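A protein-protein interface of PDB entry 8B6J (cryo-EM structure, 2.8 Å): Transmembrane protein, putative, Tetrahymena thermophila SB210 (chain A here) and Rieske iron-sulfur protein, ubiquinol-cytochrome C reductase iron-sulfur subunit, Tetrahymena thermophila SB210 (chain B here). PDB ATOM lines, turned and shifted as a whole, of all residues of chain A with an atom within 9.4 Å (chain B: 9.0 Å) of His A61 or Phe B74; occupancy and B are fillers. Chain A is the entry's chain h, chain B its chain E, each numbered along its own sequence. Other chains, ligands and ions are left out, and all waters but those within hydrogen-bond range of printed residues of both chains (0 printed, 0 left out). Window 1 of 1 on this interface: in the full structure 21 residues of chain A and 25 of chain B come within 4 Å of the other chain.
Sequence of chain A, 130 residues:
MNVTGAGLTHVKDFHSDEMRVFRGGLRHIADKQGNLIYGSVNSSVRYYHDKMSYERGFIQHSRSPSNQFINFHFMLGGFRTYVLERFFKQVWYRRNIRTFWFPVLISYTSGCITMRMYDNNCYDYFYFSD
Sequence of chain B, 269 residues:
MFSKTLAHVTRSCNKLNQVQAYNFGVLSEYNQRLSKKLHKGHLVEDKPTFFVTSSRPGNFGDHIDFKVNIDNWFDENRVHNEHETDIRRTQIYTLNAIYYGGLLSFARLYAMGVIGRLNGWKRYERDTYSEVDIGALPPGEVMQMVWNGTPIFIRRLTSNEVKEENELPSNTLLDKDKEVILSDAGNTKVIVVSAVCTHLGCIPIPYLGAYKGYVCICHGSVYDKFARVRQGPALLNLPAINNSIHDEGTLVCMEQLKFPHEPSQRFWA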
ATOM      1  N   PHE A  58      14.255 -36.902   7.116  1.00  0.00           N
ATOM      2  CA  PHE A  58      14.357 -36.174   8.372  1.00  0.00           C
ATOM      3  C   PHE A  58      15.467 -35.140   8.263  1.00  0.00           C
ATOM      4  O   PHE A  58      16.591 -35.469   7.873  1.00  0.00           O
ATOM      5  CB  PHE A  58      14.635 -37.130   9.535  1.00  0.00           C
ATOM      6  CG  PHE A  58      14.807 -36.440  10.857  1.00  0.00           C
ATOM      7  CD1 PHE A  58      13.708 -36.109  11.628  1.00  0.00           C
ATOM      8  CD2 PHE A  58      16.069 -36.122  11.328  1.00  0.00           C
ATOM      9  CE1 PHE A  58      13.864 -35.474  12.844  1.00  0.00           C
ATOM     10  CE2 PHE A  58      16.229 -35.488  12.543  1.00  0.00           C
ATOM     11  CZ  PHE A  58      15.125 -35.164  13.301  1.00  0.00           C
ATOM     12  N   ILE A  59      15.149 -33.895   8.604  1.00  0.00           N
ATOM     13  CA  ILE A  59      16.103 -32.795   8.583  1.00  0.00           C
ATOM     14  C   ILE A  59      16.046 -32.100   9.933  1.00  0.00           C
ATOM     15  O   ILE A  59      14.955 -31.817  10.441  1.00  0.00           O
ATOM     16  CB  ILE A  59      15.802 -31.794   7.450  1.00  0.00           C
ATOM     17  CG1 ILE A  59      15.749 -32.514   6.103  1.00  0.00           C
ATOM     18  CG2 ILE A  59      16.853 -30.692   7.418  1.00  0.00           C
ATOM     19  CD1 ILE A  59      15.463 -31.603   4.933  1.00  0.00           C
ATOM     20  N   GLN A  60      17.211 -31.832  10.518  1.00  0.00           N
ATOM     21  CA  GLN A  60      17.294 -31.054  11.743  1.00  0.00           C
ATOM     22  C   GLN A  60      18.271 -29.905  11.548  1.00  0.00           C
ATOM     23  O   GLN A  60      19.247 -30.017  10.801  1.00  0.00           O
ATOM     24  CB  GLN A  60      17.718 -31.907  12.951  1.00  0.00           C
ATOM     25  CG  GLN A  60      19.183 -32.306  12.998  1.00  0.00           C
ATOM     26  CD  GLN A  60      19.601 -32.770  14.376  1.00  0.00           C
ATOM     27  OE1 GLN A  60      20.623 -32.336  14.904  1.00  0.00           O
ATOM     28  NE2 GLN A  60      18.810 -33.655  14.969  1.00  0.00           N
ATOM     29  N   HIS A  61      18.001 -28.801  12.235  1.00  0.00           N
ATOM     30  CA  HIS A  61      18.807 -27.595  12.150  1.00  0.00           C
ATOM     31  C   HIS A  61      19.349 -27.246  13.527  1.00  0.00           C
ATOM     32  O   HIS A  61      18.624 -27.315  14.525  1.00  0.00           O
ATOM     33  CB  HIS A  61      17.990 -26.420  11.606  1.00  0.00           C
ATOM     34  CG  HIS A  61      17.300 -26.715  10.312  1.00  0.00           C
ATOM     35  ND1 HIS A  61      17.827 -26.357   9.090  1.00  0.00           N
ATOM     36  CD2 HIS A  61      16.125 -27.333  10.049  1.00  0.00           C
ATOM     37  CE1 HIS A  61      17.006 -26.742   8.129  1.00  0.00           C
ATOM     38  NE2 HIS A  61      15.966 -27.336   8.684  1.00  0.00           N
ATOM     39  N   SER A  62      20.624 -26.877  13.577  1.00  0.00           N
ATOM     40  CA  SER A  62      21.262 -26.431  14.804  1.00  0.00           C
ATOM     41  C   SER A  62      22.041 -25.156  14.525  1.00  0.00           C
ATOM     42  O   SER A  62      22.563 -24.956  13.426  1.00  0.00           O
ATOM     43  CB  SER A  62      22.192 -27.504  15.380  1.00  0.00           C
ATOM     44  OG  SER A  62      23.190 -27.863  14.445  1.00  0.00           O
ATOM     45  N   ARG A  63      22.116 -24.297  15.535  1.00  0.00           N
ATOM     46  CA  ARG A  63      22.732 -22.987  15.410  1.00  0.00           C
ATOM     47  C   ARG A  63      23.947 -22.900  16.321  1.00  0.00           C
ATOM     48  O   ARG A  63      23.992 -23.524  17.386  1.00  0.00           O
ATOM     49  CB  ARG A  63      21.735 -21.876  15.758  1.00  0.00           C
ATOM     50  CG  ARG A  63      22.205 -20.478  15.398  1.00  0.00           C
ATOM     51  CD  ARG A  63      21.178 -19.428  15.795  1.00  0.00           C
ATOM     52  NE  ARG A  63      19.867 -19.686  15.211  1.00  0.00           N
ATOM     53  CZ  ARG A  63      19.512 -19.348  13.979  1.00  0.00           C
ATOM     54  NH1 ARG A  63      20.353 -18.747  13.155  1.00  0.00           N
ATOM     55  NH2 ARG A  63      18.279 -19.623  13.563  1.00  0.00           N
ATOM     56  N   SER A  64      24.933 -22.123  15.893  1.00  0.00           N
ATOM     57  CA  SER A  64      26.131 -21.939  16.695  1.00  0.00           C
ATOM     58  C   SER A  64      25.766 -21.260  18.013  1.00  0.00           C
ATOM     59  O   SER A  64      25.004 -20.284  18.009  1.00  0.00           O
ATOM     60  CB  SER A  64      27.156 -21.098  15.938  1.00  0.00           C
ATOM     61  OG  SER A  64      28.289 -20.831  16.744  1.00  0.00           O
ATOM     62  N   ASN A  67      25.723 -17.390  18.464  1.00  0.00           N
ATOM     63  CA  ASN A  67      24.578 -16.595  18.044  1.00  0.00           C
ATOM     64  C   ASN A  67      23.373 -16.756  18.961  1.00  0.00           C
ATOM     65  O   ASN A  67      22.310 -16.203  18.664  1.00  0.00           O
ATOM     66  CB  ASN A  67      24.182 -16.963  16.611  1.00  0.00           C
ATOM     67  CG  ASN A  67      25.272 -16.657  15.607  1.00  0.00           C
ATOM     68  OD1 ASN A  67      25.713 -17.533  14.866  1.00  0.00           O
ATOM     69  ND2 ASN A  67      25.713 -15.405  15.576  1.00  0.00           N
ATOM     70  N   GLN A  68      23.510 -17.492  20.060  1.00  0.00           N
ATOM     71  CA  GLN A  68      22.411 -17.770  20.970  1.00  0.00           C
ATOM     72  C   GLN A  68      22.687 -17.142  22.331  1.00  0.00           C
ATOM     73  O   GLN A  68      23.820 -16.783  22.655  1.00  0.00           O
ATOM     74  CB  GLN A  68      22.195 -19.280  21.122  1.00  0.00           C
ATOM     75  CG  GLN A  68      21.848 -19.981  19.820  1.00  0.00           C
ATOM     76  CD  GLN A  68      21.595 -21.461  20.004  1.00  0.00           C
ATOM     77  OE1 GLN A  68      22.205 -22.107  20.854  1.00  0.00           O
ATOM     78  NE2 GLN A  68      20.682 -22.006  19.211  1.00  0.00           N
ATOM     79  N   PHE A  69      21.628 -17.015  23.126  1.00  0.00           N
ATOM     80  CA  PHE A  69      21.760 -16.445  24.459  1.00  0.00           C
ATOM     81  C   PHE A  69      22.739 -17.260  25.295  1.00  0.00           C
ATOM     82  O   PHE A  69      22.760 -18.492  25.230  1.00  0.00           O
ATOM     83  CB  PHE A  69      20.400 -16.404  25.159  1.00  0.00           C
ATOM     84  CG  PHE A  69      19.471 -15.348  24.632  1.00  0.00           C
ATOM     85  CD1 PHE A  69      18.605 -15.625  23.590  1.00  0.00           C
ATOM     86  CD2 PHE A  69      19.453 -14.083  25.192  1.00  0.00           C
ATOM     87  CE1 PHE A  69      17.746 -14.657  23.110  1.00  0.00           C
ATOM     88  CE2 PHE A  69      18.596 -13.112  24.715  1.00  0.00           C
ATOM     89  CZ  PHE A  69      17.742 -13.401  23.673  1.00  0.00           C
ATOM     90  N   PHE A  72      19.760 -18.682  28.185  1.00  0.00           N
ATOM     91  CA  PHE A  72      18.456 -18.544  27.556  1.00  0.00           C
ATOM     92  C   PHE A  72      17.338 -18.928  28.518  1.00  0.00           C
ATOM     93  O   PHE A  72      17.486 -19.823  29.354  1.00  0.00           O
ATOM     94  CB  PHE A  72      18.371 -19.416  26.301  1.00  0.00           C
ATOM     95  CG  PHE A  72      17.015 -19.416  25.655  1.00  0.00           C
ATOM     96  CD1 PHE A  72      16.490 -18.255  25.114  1.00  0.00           C
ATOM     97  CD2 PHE A  72      16.267 -20.578  25.583  1.00  0.00           C
ATOM     98  CE1 PHE A  72      15.243 -18.253  24.520  1.00  0.00           C
ATOM     99  CE2 PHE A  72      15.022 -20.580  24.988  1.00  0.00           C
ATOM    100  CZ  PHE A  72      14.511 -19.417  24.456  1.00  0.00           C
ATOM    101  N   LEU B  43       8.364 -21.014  27.535  1.00  0.00           N
ATOM    102  CA  LEU B  43       8.174 -20.275  26.290  1.00  0.00           C
ATOM    103  C   LEU B  43       8.061 -21.288  25.159  1.00  0.00           C
ATOM    104  O   LEU B  43       9.057 -21.732  24.587  1.00  0.00           O
ATOM    105  CB  LEU B  43       9.325 -19.303  26.061  1.00  0.00           C
ATOM    106  CG  LEU B  43       9.253 -18.463  24.785  1.00  0.00           C
ATOM    107  CD1 LEU B  43       8.034 -17.558  24.800  1.00  0.00           C
ATOM    108  CD2 LEU B  43      10.525 -17.653  24.617  1.00  0.00           C
ATOM    109  N   GLU B  45       5.410 -22.730  21.690  1.00  0.00           N
ATOM    110  CA  GLU B  45       4.446 -22.311  20.686  1.00  0.00           C
ATOM    111  C   GLU B  45       3.024 -22.579  21.162  1.00  0.00           C
ATOM    112  O   GLU B  45       2.730 -23.633  21.731  1.00  0.00           O
ATOM    113  CB  GLU B  45       4.700 -23.048  19.373  1.00  0.00           C
ATOM    114  CG  GLU B  45       6.082 -22.825  18.792  1.00  0.00           C
ATOM    115  CD  GLU B  45       6.366 -23.733  17.615  1.00  0.00           C
ATOM    116  OE1 GLU B  45       5.540 -24.629  17.340  1.00  0.00           O
ATOM    117  OE2 GLU B  45       7.414 -23.555  16.960  1.00  0.00           O
ATOM    118  N   PHE B  51       7.831 -26.121   9.413  1.00  0.00           N
ATOM    119  CA  PHE B  51       8.890 -25.483   8.644  1.00  0.00           C
ATOM    120  C   PHE B  51       9.435 -26.486   7.639  1.00  0.00           C
ATOM    121  O   PHE B  51       9.743 -27.626   8.003  1.00  0.00           O
ATOM    122  CB  PHE B  51      10.009 -24.985   9.562  1.00  0.00           C
ATOM    123  CG  PHE B  51       9.530 -24.094  10.672  1.00  0.00           C
ATOM    124  CD1 PHE B  51       9.066 -24.633  11.859  1.00  0.00           C
ATOM    125  CD2 PHE B  51       9.547 -22.717  10.529  1.00  0.00           C
ATOM    126  CE1 PHE B  51       8.624 -23.815  12.880  1.00  0.00           C
ATOM    127  CE2 PHE B  51       9.107 -21.895  11.549  1.00  0.00           C
ATOM    128  CZ  PHE B  51       8.644 -22.445  12.724  1.00  0.00           C
ATOM    129  N   VAL B  52       9.548 -26.066   6.382  1.00  0.00           N
ATOM    130  CA  VAL B  52      10.042 -26.915   5.305  1.00  0.00           C
ATOM    131  C   VAL B  52      11.229 -26.221   4.654  1.00  0.00           C
ATOM    132  O   VAL B  52      11.153 -25.034   4.319  1.00  0.00           O
ATOM    133  CB  VAL B  52       8.947 -27.216   4.265  1.00  0.00           C
ATOM    134  CG1 VAL B  52       7.736 -27.832   4.938  1.00  0.00           C
ATOM    135  CG2 VAL B  52       8.561 -25.956   3.510  1.00  0.00           C
ATOM    136  N   THR B  53      12.323 -26.958   4.486  1.00  0.00           N
ATOM    137  CA  THR B  53      13.492 -26.439   3.790  1.00  0.00           C
ATOM    138  C   THR B  53      13.214 -26.426   2.293  1.00  0.00           C
ATOM    139  O   THR B  53      12.899 -27.466   1.705  1.00  0.00           O
ATOM    140  CB  THR B  53      14.723 -27.285   4.102  1.00  0.00           C
ATOM    141  OG1 THR B  53      14.423 -28.666   3.880  1.00  0.00           O
ATOM    142  CG2 THR B  53      15.150 -27.094   5.540  1.00  0.00           C
ATOM    143  N   SER B  54      13.328 -25.249   1.677  1.00  0.00           N
ATOM    144  CA  SER B  54      13.008 -25.120   0.262  1.00  0.00           C
ATOM    145  C   SER B  54      13.984 -25.874  -0.628  1.00  0.00           C
ATOM    146  O   SER B  54      13.625 -26.227  -1.756  1.00  0.00           O
ATOM    147  CB  SER B  54      12.984 -23.643  -0.129  1.00  0.00           C
ATOM    148  OG  SER B  54      14.163 -22.988   0.300  1.00  0.00           O
ATOM    149  N   SER B  55      15.200 -26.136  -0.150  1.00  0.00           N
ATOM    150  CA  SER B  55      16.236 -26.781  -0.945  1.00  0.00           C
ATOM    151  C   SER B  55      16.469 -28.226  -0.516  1.00  0.00           C
ATOM    152  O   SER B  55      17.578 -28.746  -0.643  1.00  0.00           O
ATOM    153  CB  SER B  55      17.538 -25.987  -0.857  1.00  0.00           C
ATOM    154  OG  SER B  55      18.497 -26.492  -1.769  1.00  0.00           O
ATOM    155  N   ARG B  56      15.432 -28.884  -0.005  1.00  0.00           N
ATOM    156  CA  ARG B  56      15.552 -30.270   0.401  1.00  0.00           C
ATOM    157  C   ARG B  56      15.616 -31.175  -0.827  1.00  0.00           C
ATOM    158  O   ARG B  56      15.283 -30.758  -1.938  1.00  0.00           O
ATOM    159  CB  ARG B  56      14.374 -30.665   1.287  1.00  0.00           C
ATOM    160  CG  ARG B  56      13.111 -31.020   0.524  1.00  0.00           C
ATOM    161  CD  ARG B  56      11.909 -31.102   1.442  1.00  0.00           C
ATOM    162  NE  ARG B  56      11.196 -29.833   1.515  1.00  0.00           N
ATOM    163  CZ  ARG B  56      10.185 -29.491   0.727  1.00  0.00           C
ATOM    164  NH1 ARG B  56       9.726 -30.308  -0.207  1.00  0.00           N
ATOM    165  NH2 ARG B  56       9.621 -28.297   0.880  1.00  0.00           N
ATOM    166  N   ASN B  69       7.817 -30.364  16.405  1.00  0.00           N
ATOM    167  CA  ASN B  69       8.300 -29.285  17.257  1.00  0.00           C
ATOM    168  C   ASN B  69       7.167 -28.731  18.109  1.00  0.00           C
ATOM    169  O   ASN B  69       6.095 -28.402  17.590  1.00  0.00           O
ATOM    170  CB  ASN B  69       8.907 -28.160  16.418  1.00  0.00           C
ATOM    171  CG  ASN B  69      10.199 -28.564  15.744  1.00  0.00           C
ATOM    172  OD1 ASN B  69      11.022 -29.272  16.325  1.00  0.00           O
ATOM    173  ND2 ASN B  69      10.387 -28.114  14.511  1.00  0.00           N
ATOM    174  N   ILE B  70       7.411 -28.627  19.415  1.00  0.00           N
ATOM    175  CA  ILE B  70       6.517 -27.895  20.304  1.00  0.00           C
ATOM    176  C   ILE B  70       7.051 -26.501  20.619  1.00  0.00           C
ATOM    177  O   ILE B  70       6.256 -25.607  20.945  1.00  0.00           O
ATOM    178  CB  ILE B  70       6.273 -28.672  21.616  1.00  0.00           C
ATOM    179  CG1 ILE B  70       5.575 -30.003  21.321  1.00  0.00           C
ATOM    180  CG2 ILE B  70       5.452 -27.828  22.588  1.00  0.00           C
ATOM    181  CD1 ILE B  70       5.364 -30.878  22.540  1.00  0.00           C
ATOM    182  N   ASP B  71       8.361 -26.289  20.524  1.00  0.00           N
ATOM    183  CA  ASP B  71       8.985 -25.013  20.834  1.00  0.00           C
ATOM    184  C   ASP B  71       9.643 -24.438  19.588  1.00  0.00           C
ATOM    185  O   ASP B  71      10.083 -25.175  18.701  1.00  0.00           O
ATOM    186  CB  ASP B  71      10.036 -25.159  21.937  1.00  0.00           C
ATOM    187  CG  ASP B  71       9.468 -25.746  23.207  1.00  0.00           C
ATOM    188  OD1 ASP B  71       8.335 -26.266  23.165  1.00  0.00           O
ATOM    189  OD2 ASP B  71      10.153 -25.686  24.248  1.00  0.00           O
ATOM    190  N   ASN B  72       9.708 -23.112  19.534  1.00  0.00           N
ATOM    191  CA  ASN B  72      10.397 -22.389  18.471  1.00  0.00           C
ATOM    192  C   ASN B  72      11.716 -21.816  18.980  1.00  0.00           C
ATOM    193  O   ASN B  72      12.131 -20.724  18.589  1.00  0.00           O
ATOM    194  CB  ASN B  72       9.513 -21.281  17.908  1.00  0.00           C
ATOM    195  CG  ASN B  72      10.018 -20.747  16.584  1.00  0.00           C
ATOM    196  OD1 ASN B  72      10.749 -21.427  15.866  1.00  0.00           O
ATOM    197  ND2 ASN B  72       9.630 -19.522  16.253  1.00  0.00           N
ATOM    198  N   TRP B  73      12.389 -22.553  19.866  1.00  0.00           N
ATOM    199  CA  TRP B  73      13.638 -22.070  20.441  1.00  0.00           C
ATOM    200  C   TRP B  73      14.725 -21.881  19.393  1.00  0.00           C
ATOM    201  O   TRP B  73      15.670 -21.122  19.629  1.00  0.00           O
ATOM    202  CB  TRP B  73      14.134 -23.034  21.519  1.00  0.00           C
ATOM    203  CG  TRP B  73      13.291 -23.053  22.756  1.00  0.00           C
ATOM    204  CD1 TRP B  73      12.163 -22.325  22.992  1.00  0.00           C
ATOM    205  CD2 TRP B  73      13.513 -23.841  23.930  1.00  0.00           C
ATOM    206  NE1 TRP B  73      11.667 -22.612  24.239  1.00  0.00           N
ATOM    207  CE2 TRP B  73      12.479 -23.540  24.837  1.00  0.00           C
ATOM    208  CE3 TRP B  73      14.486 -24.773  24.302  1.00  0.00           C
ATOM    209  CZ2 TRP B  73      12.390 -24.137  26.091  1.00  0.00           C
ATOM    210  CZ3 TRP B  73      14.395 -25.366  25.548  1.00  0.00           C
ATOM    211  CH2 TRP B  73      13.355 -25.045  26.427  1.00  0.00           C
ATOM    212  N   PHE B  74      14.619 -22.551  18.243  1.00  0.00           N
ATOM    213  CA  PHE B  74      15.624 -22.371  17.203  1.00  0.00           C
ATOM    214  C   PHE B  74      15.706 -20.917  16.760  1.00  0.00           C
ATOM    215  O   PHE B  74      16.786 -20.437  16.399  1.00  0.00           O
ATOM    216  CB  PHE B  74      15.317 -23.276  16.011  1.00  0.00           C
ATOM    217  CG  PHE B  74      16.355 -23.223  14.928  1.00  0.00           C
ATOM    218  CD1 PHE B  74      17.563 -23.880  15.077  1.00  0.00           C
ATOM    219  CD2 PHE B  74      16.122 -22.521  13.762  1.00  0.00           C
ATOM    220  CE1 PHE B  74      18.518 -23.832  14.082  1.00  0.00           C
ATOM    221  CE2 PHE B  74      17.073 -22.472  12.763  1.00  0.00           C
ATOM    222  CZ  PHE B  74      18.271 -23.128  12.924  1.00  0.00           C
ATOM    223  N   ASP B  75      14.580 -20.204  16.782  1.00  0.00           N
ATOM    224  CA  ASP B  75      14.535 -18.785  16.452  1.00  0.00           C
ATOM    225  C   ASP B  75      14.463 -17.891  17.681  1.00  0.00           C
ATOM    226  O   ASP B  75      15.117 -16.846  17.719  1.00  0.00           O
ATOM    227  CB  ASP B  75      13.336 -18.491  15.547  1.00  0.00           C
ATOM    228  CG  ASP B  75      13.511 -19.048  14.150  1.00  0.00           C
ATOM    229  OD1 ASP B  75      14.664 -19.118  13.675  1.00  0.00           O
ATOM    230  OD2 ASP B  75      12.495 -19.414  13.524  1.00  0.00           O
ATOM    231  N   GLU B  76      13.677 -18.275  18.689  1.00  0.00           N
ATOM    232  CA  GLU B  76      13.570 -17.451  19.889  1.00  0.00           C
ATOM    233  C   GLU B  76      14.905 -17.353  20.613  1.00  0.00           C
ATOM    234  O   GLU B  76      15.282 -16.277  21.092  1.00  0.00           O
ATOM    235  CB  GLU B  76      12.496 -18.018  20.815  1.00  0.00           C
ATOM    236  CG  GLU B  76      11.090 -17.900  20.259  1.00  0.00           C
ATOM    237  CD  GLU B  76      10.067 -18.615  21.112  1.00  0.00           C
ATOM    238  OE1 GLU B  76      10.476 -19.365  22.023  1.00  0.00           O
ATOM    239  OE2 GLU B  76       8.855 -18.430  20.873  1.00  0.00           O
ATOM    240  N   ASN B  77      15.637 -18.464  20.704  1.00  0.00           N
ATOM    241  CA  ASN B  77      16.941 -18.485  21.367  1.00  0.00           C
ATOM    242  C   ASN B  77      17.983 -17.892  20.418  1.00  0.00           C
ATOM    243  O   ASN B  77      18.853 -18.575  19.876  1.00  0.00           O
ATOM    244  CB  ASN B  77      17.306 -19.903  21.782  1.00  0.00           C
ATOM    245  CG  ASN B  77      18.537 -19.954  22.666  1.00  0.00           C
ATOM    246  OD1 ASN B  77      19.308 -19.000  22.729  1.00  0.00           O
ATOM    247  ND2 ASN B  77      18.726 -21.073  23.350  1.00  0.00           N
ATOM    248  N   ARG B  78      17.875 -16.580  20.221  1.00  0.00           N
ATOM    249  CA  ARG B  78      18.749 -15.875  19.294  1.00  0.00           C
ATOM    250  C   ARG B  78      19.012 -14.466  19.793  1.00  0.00           C
ATOM    251  O   ARG B  78      18.072 -13.722  20.084  1.00  0.00           O
ATOM    252  CB  ARG B  78      18.133 -15.804  17.894  1.00  0.00           C
ATOM    253  CG  ARG B  78      18.061 -17.121  17.160  1.00  0.00           C
ATOM    254  CD  ARG B  78      17.595 -16.900  15.733  1.00  0.00           C
ATOM    255  NE  ARG B  78      18.531 -16.068  14.987  1.00  0.00           N
ATOM    256  CZ  ARG B  78      18.309 -15.592  13.769  1.00  0.00           C
ATOM    257  NH1 ARG B  78      17.177 -15.833  13.128  1.00  0.00           N
ATOM    258  NH2 ARG B  78      19.246 -14.856  13.180  1.00  0.00           N
ATOM    259  N   VAL B  79      20.287 -14.110  19.886  1.00  0.00           N
ATOM    260  CA  VAL B  79      20.714 -12.718  19.947  1.00  0.00           C
ATOM    261  C   VAL B  79      21.208 -12.377  18.548  1.00  0.00           C
ATOM    262  O   VAL B  79      22.231 -12.898  18.093  1.00  0.00           O
ATOM    263  CB  VAL B  79      21.793 -12.491  21.014  1.00  0.00           C
ATOM    264  CG1 VAL B  79      21.289 -12.934  22.378  1.00  0.00           C
ATOM    265  CG2 VAL B  79      23.081 -13.218  20.659  1.00  0.00           C
ATOM    266  N   HIS B  80      20.472 -11.520  17.844  1.00  0.00           N
ATOM    267  CA  HIS B  80      20.695 -11.323  16.413  1.00  0.00           C
ATOM    268  C   HIS B  80      21.976 -10.518  16.223  1.00  0.00           C
ATOM    269  O   HIS B  80      21.969  -9.314  15.955  1.00  0.00           O
ATOM    270  CB  HIS B  80      19.491 -10.645  15.776  1.00  0.00           C
ATOM    271  CG  HIS B  80      18.241 -11.464  15.846  1.00  0.00           C
ATOM    272  ND1 HIS B  80      17.493 -11.583  16.997  1.00  0.00           N
ATOM    273  CD2 HIS B  80      17.617 -12.220  14.913  1.00  0.00           C
ATOM    274  CE1 HIS B  80      16.457 -12.369  16.767  1.00  0.00           C
ATOM    275  NE2 HIS B  80      16.508 -12.768  15.511  1.00  0.00           N
ATOM    276  N   GLU B  82      24.606 -11.743  14.068  1.00  0.00           N
ATOM    277  CA  GLU B  82      25.334 -12.415  12.997  1.00  0.00           C
ATOM    278  C   GLU B  82      26.534 -11.594  12.555  1.00  0.00           C
ATOM    279  O   GLU B  82      27.532 -12.150  12.083  1.00  0.00           O
ATOM    280  CB  GLU B  82      24.404 -12.691  11.817  1.00  0.00           C
ATOM    281  CG  GLU B  82      23.523 -13.917  12.003  1.00  0.00           C
ATOM    282  CD  GLU B  82      22.621 -13.813  13.217  1.00  0.00           C
ATOM    283  OE1 GLU B  82      22.455 -12.691  13.738  1.00  0.00           O
ATOM    284  OE2 GLU B  82      22.080 -14.852  13.650  1.00  0.00           O
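CG2 of Thr B53 touches CE1 of His A61, 3.2 Å away.
N of Ser A62 touches CE1 of Phe B74, 3.7 Å away.
Asn A67 touches Arg B78.
Asn A67 touches Glu B82 (ND2 to CA, 3.97 Å).
Gln A68 touches Asn B77.
O of Glu B76 touches CE1 of Phe A69, at 3.6 Å.
O of Arg B78 touches CE1 of Phe A69 (3.2 Å).
Val B79 touches Phe A69.
Phe A72 touches Glu B76.
Phe A72 touches Asn B77 (CG to ND2, 3.3 Å).
The backbone carbonyl oxygen of Phe B74 lies close to the guanidinium group of Arg A63 (3.3 Å).
OD1 of Asn B77 sits at hydrogen-bond distance from N of Phe A69, at 3.1 Å.
The side-chain carboxylate (OD1) of Asp B75 is in salt-bridge range of the guanidinium group (NH2) of Arg A63, 3.7 Å away.
N of Val B79 lies within hydrogen-bond range of O of Asn A67 (3.2 Å).
Of the 21 printed residues of chain B, 10 touch a printed residue of chain A.
Of the 11 printed residues of chain A, 8 touch a printed residue of chain B.
Hydrophobic or aromatic side chains of chain A within 4 Å of the printed part of chain B: Ile A59, His A61, Phe A69 and Phe A72.
Along chain A the printed residues that touch a printed residue of chain B span positions 59 to 72.
Among the printed residues, 19 pairs touch across the chains.
Among the printed residues, Asp or Glu carboxylates within 4 Å of a Lys or Arg side-chain nitrogen of the other chain: Arg A63 with Asp B75.
His A61 touches two residues of chain B.
Of chain A, only His A61 (3.5 Å), Ser A62 (3.7 Å) and Arg A63 (3.2 Å) come within 4 Å of Phe B74.
Asp B75 touches just one residue of chain A: Arg A63.
Of the printed residues of chain A, Arg B78 touches Arg A63 (3.5 Å), Asn A67 (3.6 Å) and Phe A69 (3.2 Å).
Of the printed residues of chain B, Phe A72 touches Trp B73, Glu B76 and Asn B77.
Of the printed residues of chain B, Ile A59 touches Thr B53 and Arg B56.
Of the printed residues of chain A, Val B79 touches Asn A67 (3.2 Å) and Phe A69 (3.6 Å).
Asp B71 touches none of the printed residues of chain A.
The nearest residue of chain B that does not touch His A61 is Phe B51 (6.3 Å).
The nearest residue of chain A that does not touch Phe B74 is Gln A68 (5.1 Å).
The guanidinium group (NH2) of Arg B78 is in salt-bridge range of the side-chain carboxylate (OE2) of Glu B82 (2.9 Å).
O of Leu B43 lies within hydrogen-bond range of NE1 of Trp B73 (2.8 Å).
The side-chain carboxylate (OD2) of Asp B71 sits close to the indole nitrogen (NE1) of Trp B73, at 3.4 Å.
The guanidinium group (NE) of Arg B56 lies within hydrogen-bond range of the backbone carbonyl oxygen (O) of Thr B53 (2.9 Å).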
